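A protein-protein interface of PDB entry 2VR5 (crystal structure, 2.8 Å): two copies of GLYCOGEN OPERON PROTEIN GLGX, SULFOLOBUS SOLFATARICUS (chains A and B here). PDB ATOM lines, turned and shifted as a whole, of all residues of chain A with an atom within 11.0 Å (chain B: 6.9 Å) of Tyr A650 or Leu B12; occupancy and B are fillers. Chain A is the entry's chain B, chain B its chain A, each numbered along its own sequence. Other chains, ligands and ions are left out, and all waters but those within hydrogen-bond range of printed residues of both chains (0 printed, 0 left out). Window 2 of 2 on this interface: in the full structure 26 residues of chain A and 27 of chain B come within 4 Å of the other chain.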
ATOM      1  N   LYS A 167      -5.172  -0.462  -0.921  1.00  0.00           N
ATOM      2  CA  LYS A 167      -4.466  -1.567  -1.559  1.00  0.00           C
ATOM      3  C   LYS A 167      -5.254  -2.867  -1.440  1.00  0.00           C
ATOM      4  O   LYS A 167      -6.043  -3.043  -0.512  1.00  0.00           O
ATOM      5  CB  LYS A 167      -3.074  -1.738  -0.947  1.00  0.00           C
ATOM      6  CG  LYS A 167      -3.086  -2.136   0.519  1.00  0.00           C
ATOM      7  CD  LYS A 167      -1.916  -1.518   1.269  1.00  0.00           C
ATOM      8  CE  LYS A 167      -0.588  -1.957   0.677  1.00  0.00           C
ATOM      9  NZ  LYS A 167       0.551  -1.167   1.222  1.00  0.00           N
ATOM     10  N   PRO A 170      -1.960  -7.749  -4.457  1.00  0.00           N
ATOM     11  CA  PRO A 170      -1.175  -7.534  -5.677  1.00  0.00           C
ATOM     12  C   PRO A 170      -0.891  -8.842  -6.406  1.00  0.00           C
ATOM     13  O   PRO A 170      -0.661  -9.867  -5.766  1.00  0.00           O
ATOM     14  CB  PRO A 170       0.128  -6.932  -5.147  1.00  0.00           C
ATOM     15  CG  PRO A 170       0.253  -7.477  -3.769  1.00  0.00           C
ATOM     16  CD  PRO A 170      -1.149  -7.579  -3.239  1.00  0.00           C
ATOM     17  N   LYS A 172       1.441 -10.120  -7.517  1.00  0.00           N
ATOM     18  CA  LYS A 172       2.703 -10.746  -7.142  1.00  0.00           C
ATOM     19  C   LYS A 172       2.478 -11.894  -6.163  1.00  0.00           C
ATOM     20  O   LYS A 172       3.166 -12.914  -6.219  1.00  0.00           O
ATOM     21  CB  LYS A 172       3.653  -9.713  -6.532  1.00  0.00           C
ATOM     22  CG  LYS A 172       5.112 -10.138  -6.530  1.00  0.00           C
ATOM     23  CD  LYS A 172       5.974  -9.151  -5.759  1.00  0.00           C
ATOM     24  CE  LYS A 172       5.863  -9.377  -4.259  1.00  0.00           C
ATOM     25  NZ  LYS A 172       4.592  -8.831  -3.708  1.00  0.00           N
ATOM     26  N   ASP A 173       1.513 -11.720  -5.266  1.00  0.00           N
ATOM     27  CA  ASP A 173       1.356 -12.615  -4.127  1.00  0.00           C
ATOM     28  C   ASP A 173       0.035 -13.375  -4.199  1.00  0.00           C
ATOM     29  O   ASP A 173      -0.367 -14.032  -3.239  1.00  0.00           O
ATOM     30  CB  ASP A 173       1.441 -11.832  -2.814  1.00  0.00           C
ATOM     31  CG  ASP A 173       2.609 -10.866  -2.788  1.00  0.00           C
ATOM     32  OD1 ASP A 173       3.765 -11.327  -2.887  1.00  0.00           O
ATOM     33  OD2 ASP A 173       2.370  -9.646  -2.666  1.00  0.00           O
ATOM     34  N   GLU A 597       8.528 -10.345  -8.665  1.00  0.00           N
ATOM     35  CA  GLU A 597       8.047  -9.336  -9.601  1.00  0.00           C
ATOM     36  C   GLU A 597       8.928  -9.273 -10.845  1.00  0.00           C
ATOM     37  O   GLU A 597       8.524  -8.740 -11.878  1.00  0.00           O
ATOM     38  CB  GLU A 597       7.991  -7.964  -8.928  1.00  0.00           C
ATOM     39  CG  GLU A 597       7.198  -6.923  -9.704  1.00  0.00           C
ATOM     40  CD  GLU A 597       6.942  -5.666  -8.897  1.00  0.00           C
ATOM     41  OE1 GLU A 597       6.317  -5.764  -7.820  1.00  0.00           O
ATOM     42  OE2 GLU A 597       7.367  -4.578  -9.339  1.00  0.00           O
ATOM     43  N   ARG A 598      10.133  -9.824 -10.738  1.00  0.00           N
ATOM     44  CA  ARG A 598      11.064  -9.851 -11.860  1.00  0.00           C
ATOM     45  C   ARG A 598      11.637 -11.250 -12.067  1.00  0.00           C
ATOM     46  O   ARG A 598      11.442 -12.140 -11.238  1.00  0.00           O
ATOM     47  CB  ARG A 598      12.197  -8.847 -11.642  1.00  0.00           C
ATOM     48  CG  ARG A 598      11.819  -7.408 -11.959  1.00  0.00           C
ATOM     49  CD  ARG A 598      13.041  -6.504 -11.958  1.00  0.00           C
ATOM     50  NE  ARG A 598      13.338  -5.988 -10.625  1.00  0.00           N
ATOM     51  CZ  ARG A 598      14.210  -5.017 -10.377  1.00  0.00           C
ATOM     52  NH1 ARG A 598      14.877  -4.452 -11.373  1.00  0.00           N
ATOM     53  NH2 ARG A 598      14.418  -4.610  -9.132  1.00  0.00           N
ATOM     54  N   GLU A 646      14.935  -8.145  -6.180  1.00  0.00           N
ATOM     55  CA  GLU A 646      13.535  -7.961  -5.818  1.00  0.00           C
ATOM     56  C   GLU A 646      13.361  -6.776  -4.874  1.00  0.00           C
ATOM     57  O   GLU A 646      13.930  -6.750  -3.782  1.00  0.00           O
ATOM     58  CB  GLU A 646      12.977  -9.232  -5.174  1.00  0.00           C
ATOM     59  CG  GLU A 646      12.267 -10.160  -6.147  1.00  0.00           C
ATOM     60  CD  GLU A 646      10.894  -9.652  -6.538  1.00  0.00           C
ATOM     61  OE1 GLU A 646      10.107  -9.303  -5.633  1.00  0.00           O
ATOM     62  OE2 GLU A 646      10.600  -9.602  -7.752  1.00  0.00           O
ATOM     63  N   ILE A 647      12.570  -5.797  -5.302  1.00  0.00           N
ATOM     64  CA  ILE A 647      12.375  -4.576  -4.528  1.00  0.00           C
ATOM     65  C   ILE A 647      10.894  -4.313  -4.276  1.00  0.00           C
ATOM     66  O   ILE A 647      10.106  -4.200  -5.214  1.00  0.00           O
ATOM     67  CB  ILE A 647      12.990  -3.355  -5.237  1.00  0.00           C
ATOM     68  CG1 ILE A 647      14.472  -3.597  -5.528  1.00  0.00           C
ATOM     69  CG2 ILE A 647      12.805  -2.101  -4.395  1.00  0.00           C
ATOM     70  CD1 ILE A 647      15.108  -2.526  -6.387  1.00  0.00           C
ATOM     71  N   ASN A 648      10.524  -4.220  -3.003  1.00  0.00           N
ATOM     72  CA  ASN A 648       9.173  -3.822  -2.626  1.00  0.00           C
ATOM     73  C   ASN A 648       8.896  -2.355  -2.938  1.00  0.00           C
ATOM     74  O   ASN A 648       9.765  -1.643  -3.440  1.00  0.00           O
ATOM     75  CB  ASN A 648       8.928  -4.099  -1.141  1.00  0.00           C
ATOM     76  CG  ASN A 648       9.762  -3.211  -0.237  1.00  0.00           C
ATOM     77  OD1 ASN A 648       9.826  -3.424   0.973  1.00  0.00           O
ATOM     78  ND2 ASN A 648      10.407  -2.210  -0.824  1.00  0.00           N
ATOM     79  N   MET A 649       7.680  -1.911  -2.637  1.00  0.00           N
ATOM     80  CA  MET A 649       7.228  -0.584  -3.036  1.00  0.00           C
ATOM     81  C   MET A 649       7.916   0.502  -2.215  1.00  0.00           C
ATOM     82  O   MET A 649       7.569   1.679  -2.310  1.00  0.00           O
ATOM     83  CB  MET A 649       5.710  -0.468  -2.892  1.00  0.00           C
ATOM     84  CG  MET A 649       5.193  -0.778  -1.496  1.00  0.00           C
ATOM     85  SD  MET A 649       3.393  -0.756  -1.400  1.00  0.00           S
ATOM     86  CE  MET A 649       3.139   0.420  -0.074  1.00  0.00           C
ATOM     87  N   TYR A 650       8.894   0.098  -1.410  1.00  0.00           N
ATOM     88  CA  TYR A 650       9.548   1.011  -0.480  1.00  0.00           C
ATOM     89  C   TYR A 650      11.034   1.148  -0.794  1.00  0.00           C
ATOM     90  O   TYR A 650      11.754   1.887  -0.123  1.00  0.00           O
ATOM     91  CB  TYR A 650       9.357   0.535   0.962  1.00  0.00           C
ATOM     92  CG  TYR A 650       7.928   0.618   1.450  1.00  0.00           C
ATOM     93  CD1 TYR A 650       7.085  -0.484   1.383  1.00  0.00           C
ATOM     94  CD2 TYR A 650       7.421   1.798   1.977  1.00  0.00           C
ATOM     95  CE1 TYR A 650       5.779  -0.412   1.828  1.00  0.00           C
ATOM     96  CE2 TYR A 650       6.117   1.879   2.425  1.00  0.00           C
ATOM     97  CZ  TYR A 650       5.300   0.772   2.348  1.00  0.00           C
ATOM     98  OH  TYR A 650       4.000   0.847   2.792  1.00  0.00           O
ATOM     99  N   GLY A 651      11.485   0.431  -1.818  1.00  0.00           N
ATOM    100  CA  GLY A 651      12.870   0.499  -2.244  1.00  0.00           C
ATOM    101  C   GLY A 651      13.780  -0.373  -1.402  1.00  0.00           C
ATOM    102  O   GLY A 651      14.987  -0.145  -1.334  1.00  0.00           O
ATOM    103  N   GLU A 652      13.195  -1.379  -0.757  1.00  0.00           N
ATOM    104  CA  GLU A 652      13.971  -2.372  -0.023  1.00  0.00           C
ATOM    105  C   GLU A 652      14.114  -3.662  -0.825  1.00  0.00           C
ATOM    106  O   GLU A 652      13.121  -4.268  -1.226  1.00  0.00           O
ATOM    107  CB  GLU A 652      13.325  -2.663   1.331  1.00  0.00           C
ATOM    108  CG  GLU A 652      13.001  -1.421   2.145  1.00  0.00           C
ATOM    109  CD  GLU A 652      12.175  -1.731   3.378  1.00  0.00           C
ATOM    110  OE1 GLU A 652      11.119  -2.384   3.241  1.00  0.00           O
ATOM    111  OE2 GLU A 652      12.581  -1.320   4.486  1.00  0.00           O
ATOM    112  N   ARG A 653      15.356  -4.076  -1.054  1.00  0.00           N
ATOM    113  CA  ARG A 653      15.639  -5.427  -1.525  1.00  0.00           C
ATOM    114  C   ARG A 653      15.269  -6.466  -0.472  1.00  0.00           C
ATOM    115  O   ARG A 653      15.394  -6.220   0.728  1.00  0.00           O
ATOM    116  CB  ARG A 653      17.114  -5.565  -1.904  1.00  0.00           C
ATOM    117  CG  ARG A 653      17.349  -6.198  -3.266  1.00  0.00           C
ATOM    118  CD  ARG A 653      18.430  -7.264  -3.200  1.00  0.00           C
ATOM    119  NE  ARG A 653      19.644  -6.773  -2.554  1.00  0.00           N
ATOM    120  CZ  ARG A 653      20.642  -7.551  -2.150  1.00  0.00           C
ATOM    121  NH1 ARG A 653      20.575  -8.864  -2.324  1.00  0.00           N
ATOM    122  NH2 ARG A 653      21.709  -7.017  -1.572  1.00  0.00           N
ATOM    123  N   ILE A 654      14.812  -7.628  -0.929  1.00  0.00           N
ATOM    124  CA  ILE A 654      13.866  -8.433  -0.165  1.00  0.00           C
ATOM    125  C   ILE A 654      14.568  -9.594   0.532  1.00  0.00           C
ATOM    126  O   ILE A 654      14.422  -9.785   1.740  1.00  0.00           O
ATOM    127  CB  ILE A 654      12.745  -8.988  -1.062  1.00  0.00           C
ATOM    128  CG1 ILE A 654      11.638  -7.946  -1.239  1.00  0.00           C
ATOM    129  CG2 ILE A 654      12.183 -10.275  -0.478  1.00  0.00           C
ATOM    130  CD1 ILE A 654      11.587  -6.917  -0.132  1.00  0.00           C
ATOM    131  N   THR B   7      23.829   6.262  -8.156  1.00  0.00           N
ATOM    132  CA  THR B   7      22.413   6.559  -8.335  1.00  0.00           C
ATOM    133  C   THR B   7      21.561   5.822  -7.308  1.00  0.00           C
ATOM    134  O   THR B   7      20.337   5.962  -7.287  1.00  0.00           O
ATOM    135  CB  THR B   7      21.932   6.185  -9.750  1.00  0.00           C
ATOM    136  OG1 THR B   7      20.528   6.444  -9.865  1.00  0.00           O
ATOM    137  CG2 THR B   7      22.197   4.714 -10.031  1.00  0.00           C
ATOM    138  N   ARG B   8      22.214   5.038  -6.457  1.00  0.00           N
ATOM    139  CA  ARG B   8      21.511   4.157  -5.532  1.00  0.00           C
ATOM    140  C   ARG B   8      21.905   4.446  -4.087  1.00  0.00           C
ATOM    141  O   ARG B   8      21.381   3.833  -3.157  1.00  0.00           O
ATOM    142  CB  ARG B   8      21.790   2.691  -5.871  1.00  0.00           C
ATOM    143  CG  ARG B   8      23.205   2.425  -6.356  1.00  0.00           C
ATOM    144  CD  ARG B   8      23.627   0.992  -6.073  1.00  0.00           C
ATOM    145  NE  ARG B   8      22.582   0.036  -6.428  1.00  0.00           N
ATOM    146  CZ  ARG B   8      22.576  -1.238  -6.049  1.00  0.00           C
ATOM    147  NH1 ARG B   8      23.562  -1.714  -5.300  1.00  0.00           N
ATOM    148  NH2 ARG B   8      21.585  -2.037  -6.418  1.00  0.00           N
ATOM    149  N   ARG B  10      21.033   7.183  -2.999  1.00  0.00           N
ATOM    150  CA  ARG B  10      20.041   8.230  -2.779  1.00  0.00           C
ATOM    151  C   ARG B  10      18.644   7.641  -2.621  1.00  0.00           C
ATOM    152  O   ARG B  10      18.123   7.002  -3.536  1.00  0.00           O
ATOM    153  CB  ARG B  10      20.062   9.237  -3.930  1.00  0.00           C
ATOM    154  CG  ARG B  10      19.143  10.432  -3.725  1.00  0.00           C
ATOM    155  CD  ARG B  10      17.950  10.378  -4.666  1.00  0.00           C
ATOM    156  NE  ARG B  10      17.126  11.579  -4.574  1.00  0.00           N
ATOM    157  CZ  ARG B  10      16.885  12.235  -3.443  1.00  0.00           C
ATOM    158  NH1 ARG B  10      17.406  11.806  -2.301  1.00  0.00           N
ATOM    159  NH2 ARG B  10      16.124  13.320  -3.453  1.00  0.00           N
ATOM    160  N   PRO B  11      18.042   7.860  -1.458  1.00  0.00           N
ATOM    161  CA  PRO B  11      16.829   7.134  -1.069  1.00  0.00           C
ATOM    162  C   PRO B  11      15.723   7.282  -2.108  1.00  0.00           C
ATOM    163  O   PRO B  11      15.421   8.397  -2.533  1.00  0.00           O
ATOM    164  CB  PRO B  11      16.420   7.820   0.236  1.00  0.00           C
ATOM    165  CG  PRO B  11      17.697   8.332   0.801  1.00  0.00           C
ATOM    166  CD  PRO B  11      18.537   8.732  -0.378  1.00  0.00           C
ATOM    167  N   LEU B  12      15.127   6.163  -2.508  1.00  0.00           N
ATOM    168  CA  LEU B  12      14.238   6.140  -3.663  1.00  0.00           C
ATOM    169  C   LEU B  12      13.235   4.995  -3.564  1.00  0.00           C
ATOM    170  O   LEU B  12      13.427   4.053  -2.797  1.00  0.00           O
ATOM    171  CB  LEU B  12      15.044   6.021  -4.958  1.00  0.00           C
ATOM    172  CG  LEU B  12      15.708   7.304  -5.463  1.00  0.00           C
ATOM    173  CD1 LEU B  12      16.349   7.079  -6.824  1.00  0.00           C
ATOM    174  CD2 LEU B  12      14.701   8.443  -5.523  1.00  0.00           C
ATOM    175  N   ARG B  13      12.164   5.085  -4.347  1.00  0.00           N
ATOM    176  CA  ARG B  13      11.235   3.971  -4.504  1.00  0.00           C
ATOM    177  C   ARG B  13      10.911   3.727  -5.974  1.00  0.00           C
ATOM    178  O   ARG B  13      11.115   4.599  -6.818  1.00  0.00           O
ATOM    179  CB  ARG B  13       9.948   4.233  -3.719  1.00  0.00           C
ATOM    180  CG  ARG B  13      10.164   4.458  -2.231  1.00  0.00           C
ATOM    181  CD  ARG B  13       8.845   4.682  -1.510  1.00  0.00           C
ATOM    182  NE  ARG B  13       9.041   5.029  -0.105  1.00  0.00           N
ATOM    183  CZ  ARG B  13       8.079   5.475   0.696  1.00  0.00           C
ATOM    184  NH1 ARG B  13       6.847   5.631   0.233  1.00  0.00           N
ATOM    185  NH2 ARG B  13       8.349   5.765   1.961  1.00  0.00           N
ATOM    186  N   PRO B  14      10.406   2.535  -6.273  1.00  0.00           N
ATOM    187  CA  PRO B  14      10.184   2.117  -7.662  1.00  0.00           C
ATOM    188  C   PRO B  14       9.071   2.921  -8.323  1.00  0.00           C
ATOM    189  O   PRO B  14       9.106   3.143  -9.533  1.00  0.00           O
ATOM    190  CB  PRO B  14       9.765   0.654  -7.518  1.00  0.00           C
ATOM    191  CG  PRO B  14       9.139   0.578  -6.171  1.00  0.00           C
ATOM    192  CD  PRO B  14       9.905   1.540  -5.308  1.00  0.00           C
ATOM    193  N   GLY B  15       8.093   3.349  -7.531  1.00  0.00           N
ATOM    194  CA  GLY B  15       7.058   4.244  -8.014  1.00  0.00           C
ATOM    195  C   GLY B  15       5.975   3.515  -8.787  1.00  0.00           C
ATOM    196  O   GLY B  15       5.874   2.290  -8.727  1.00  0.00           O
ATOM    197  N   ASP B  28       3.070   9.536   1.514  1.00  0.00           N
ATOM    198  CA  ASP B  28       4.431   9.011   1.510  1.00  0.00           C
ATOM    199  C   ASP B  28       5.454  10.132   1.361  1.00  0.00           C
ATOM    200  O   ASP B  28       6.602   9.892   0.986  1.00  0.00           O
ATOM    201  CB  ASP B  28       4.607   7.986   0.389  1.00  0.00           C
ATOM    202  CG  ASP B  28       3.550   6.899   0.421  1.00  0.00           C
ATOM    203  OD1 ASP B  28       3.613   5.981  -0.424  1.00  0.00           O
ATOM    204  OD2 ASP B  28       2.659   6.961   1.293  1.00  0.00           O
ATOM    205  N   GLU B  58      19.889  18.165  -9.130  1.00  0.00           N
ATOM    206  CA  GLU B  58      20.119  16.734  -8.974  1.00  0.00           C
ATOM    207  C   GLU B  58      19.725  15.971 -10.235  1.00  0.00           C
ATOM    208  O   GLU B  58      18.866  16.414 -10.997  1.00  0.00           O
ATOM    209  CB  GLU B  58      19.344  16.195  -7.770  1.00  0.00           C
ATOM    210  CG  GLU B  58      19.606  14.728  -7.470  1.00  0.00           C
ATOM    211  CD  GLU B  58      18.984  14.282  -6.161  1.00  0.00           C
ATOM    212  OE1 GLU B  58      19.178  13.108  -5.779  1.00  0.00           O
ATOM    213  OE2 GLU B  58      18.302  15.104  -5.513  1.00  0.00           O
ATOM    214  N   ILE B  60      18.432  12.190 -11.077  1.00  0.00           N
ATOM    215  CA  ILE B  60      18.018  10.811 -10.856  1.00  0.00           C
ATOM    216  C   ILE B  60      17.798  10.082 -12.177  1.00  0.00           C
ATOM    217  O   ILE B  60      17.228  10.637 -13.116  1.00  0.00           O
ATOM    218  CB  ILE B  60      16.727  10.736 -10.019  1.00  0.00           C
ATOM    219  CG1 ILE B  60      16.968  11.300  -8.617  1.00  0.00           C
ATOM    220  CG2 ILE B  60      16.224   9.303  -9.942  1.00  0.00           C
ATOM    221  CD1 ILE B  60      16.805  12.802  -8.527  1.00  0.00           C
ATOM    222  N   GLU B  61      18.254   8.836 -12.243  1.00  0.00           N
ATOM    223  CA  GLU B  61      17.993   7.984 -13.397  1.00  0.00           C
ATOM    224  C   GLU B  61      16.766   7.107 -13.170  1.00  0.00           C
ATOM    225  O   GLU B  61      16.778   6.215 -12.321  1.00  0.00           O
ATOM    226  CB  GLU B  61      19.211   7.113 -13.708  1.00  0.00           C
ATOM    227  CG  GLU B  61      19.187   6.481 -15.090  1.00  0.00           C
ATOM    228  CD  GLU B  61      20.218   5.380 -15.245  1.00  0.00           C
ATOM    229  OE1 GLU B  61      21.425   5.669 -15.106  1.00  0.00           O
ATOM    230  OE2 GLU B  61      19.822   4.224 -15.506  1.00  0.00           O
ATOM    231  N   VAL B  72       9.581   6.539 -11.347  1.00  0.00           N
ATOM    232  CA  VAL B  72      10.346   6.615 -10.107  1.00  0.00           C
ATOM    233  C   VAL B  72       9.602   7.423  -9.049  1.00  0.00           C
ATOM    234  O   VAL B  72       8.758   8.259  -9.373  1.00  0.00           O
ATOM    235  CB  VAL B  72      11.733   7.243 -10.337  1.00  0.00           C
ATOM    236  CG1 VAL B  72      11.593   8.683 -10.806  1.00  0.00           C
ATOM    237  CG2 VAL B  72      12.566   7.166  -9.067  1.00  0.00           C
ATOM    238  N   PHE B  73       9.920   7.167  -7.784  1.00  0.00           N
ATOM    239  CA  PHE B  73       9.400   7.972  -6.686  1.00  0.00           C
ATOM    240  C   PHE B  73      10.532   8.542  -5.836  1.00  0.00           C
ATOM    241  O   PHE B  73      11.253   7.801  -5.169  1.00  0.00           O
ATOM    242  CB  PHE B  73       8.453   7.144  -5.815  1.00  0.00           C
ATOM    243  CG  PHE B  73       7.996   7.853  -4.572  1.00  0.00           C
ATOM    244  CD1 PHE B  73       6.847   8.625  -4.583  1.00  0.00           C
ATOM    245  CD2 PHE B  73       8.716   7.747  -3.394  1.00  0.00           C
ATOM    246  CE1 PHE B  73       6.424   9.279  -3.441  1.00  0.00           C
ATOM    247  CE2 PHE B  73       8.297   8.399  -2.249  1.00  0.00           C
ATOM    248  CZ  PHE B  73       7.150   9.166  -2.273  1.00  0.00           C
ATOM    249  N   VAL B  74      10.680   9.862  -5.865  1.00  0.00           N
ATOM    250  CA  VAL B  74      11.671  10.540  -5.038  1.00  0.00           C
ATOM    251  C   VAL B  74      11.048  11.063  -3.748  1.00  0.00           C
ATOM    252  O   VAL B  74      10.131  11.885  -3.779  1.00  0.00           O
ATOM    253  CB  VAL B  74      12.329  11.711  -5.791  1.00  0.00           C
ATOM    254  CG1 VAL B  74      13.587  12.167  -5.069  1.00  0.00           C
ATOM    255  CG2 VAL B  74      12.644  11.309  -7.224  1.00  0.00           C
ATOM    256  N   PRO B  75      11.552  10.583  -2.616  1.00  0.00           N
ATOM    257  CA  PRO B  75      11.134  11.097  -1.308  1.00  0.00           C
ATOM    258  C   PRO B  75      11.524  12.559  -1.123  1.00  0.00           C
ATOM    259  O   PRO B  75      12.564  12.988  -1.624  1.00  0.00           O
ATOM    260  CB  PRO B  75      11.914  10.218  -0.328  1.00  0.00           C
ATOM    261  CG  PRO B  75      12.119   8.940  -1.059  1.00  0.00           C
ATOM    262  CD  PRO B  75      12.297   9.317  -2.503  1.00  0.00           C
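Leu B12 touches two residues of chain A. No residue of chain A comes within 4 Å of Arg B10. Arg B13 touches just these residues of chain A: Met A649 (3.4 Å) and Tyr A650 (3.7 Å). No residue of chain A comes within 4 Å of Val B74. No residue of chain A comes within 4 Å of Pro B75. Of the printed residues of chain B, Met A649 touches Arg B13 and Pro B14. Printed residues of chain B within 4 Å of Gly A651: Leu B12 (3.6 Å) and Pro B14 (3.99 Å). Of the printed residues of chain A, Pro B14 touches Asn A648 (3.6 Å), Met A649 (3.8 Å) and Gly A651 (3.99 Å). Of the printed residues of chain B, Asn A648 touches Pro B14 (3.6 Å). The nearest residue of chain B that does not touch Tyr A650 is Pro B14 (4.3 Å). The nearest residue of chain A that does not touch Leu B12 is Glu A652 (5.8 Å).
The side-chain amide nitrogen (ND2) of Asn A648 sits close to the backbone NH (N) of Gly A651, 3.0 Å away. The guanidinium group of Arg B13 lies within salt-bridge range of the side-chain carboxylate of Asp B28. The backbone carbonyl oxygen (O) of Phe B73 lies within hydrogen-bond range of the backbone NH (N) of Arg B13, at 3.0 Å. OD1 of Asn A648 lies close to OE1 of Glu A652 (2.8 Å). The backbone NH (N) of Tyr A650 sits close to the side-chain amide nitrogen (ND2) of Asn A648 (2.8 Å).
Of the 16 printed residues of chain B, 3 touch a printed residue of chain A. Hydrophobic or aromatic side chains of chain B that line the printed part of chain A: Pro B14. Printed residues of chain A that touch a printed residue of chain B: Asn A648, Met A649, Tyr A650 and Gly A651. Among the printed residues, no Asp or Glu carboxylate lies within 4 Å of a Lys or Arg side-chain nitrogen of the other chain.
Among the printed residues, pairs that only touch across the chains: Asn A648 with Pro B14 (3.6 Å), Met A649 with Arg B13 (3.4 Å), Met A649 with Pro B14 (3.8 Å), Tyr A650 with Leu B12 (3.8 Å), Tyr A650 with Arg B13 (3.7 Å), Gly A651 with Leu B12 (3.6 Å) and Gly A651 with Pro B14 (3.99 Å).
No position is printed for both chains. Of the 7 pairs that touch across the chains among the printed residues, none has its exchanged pair printed and touching as well.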
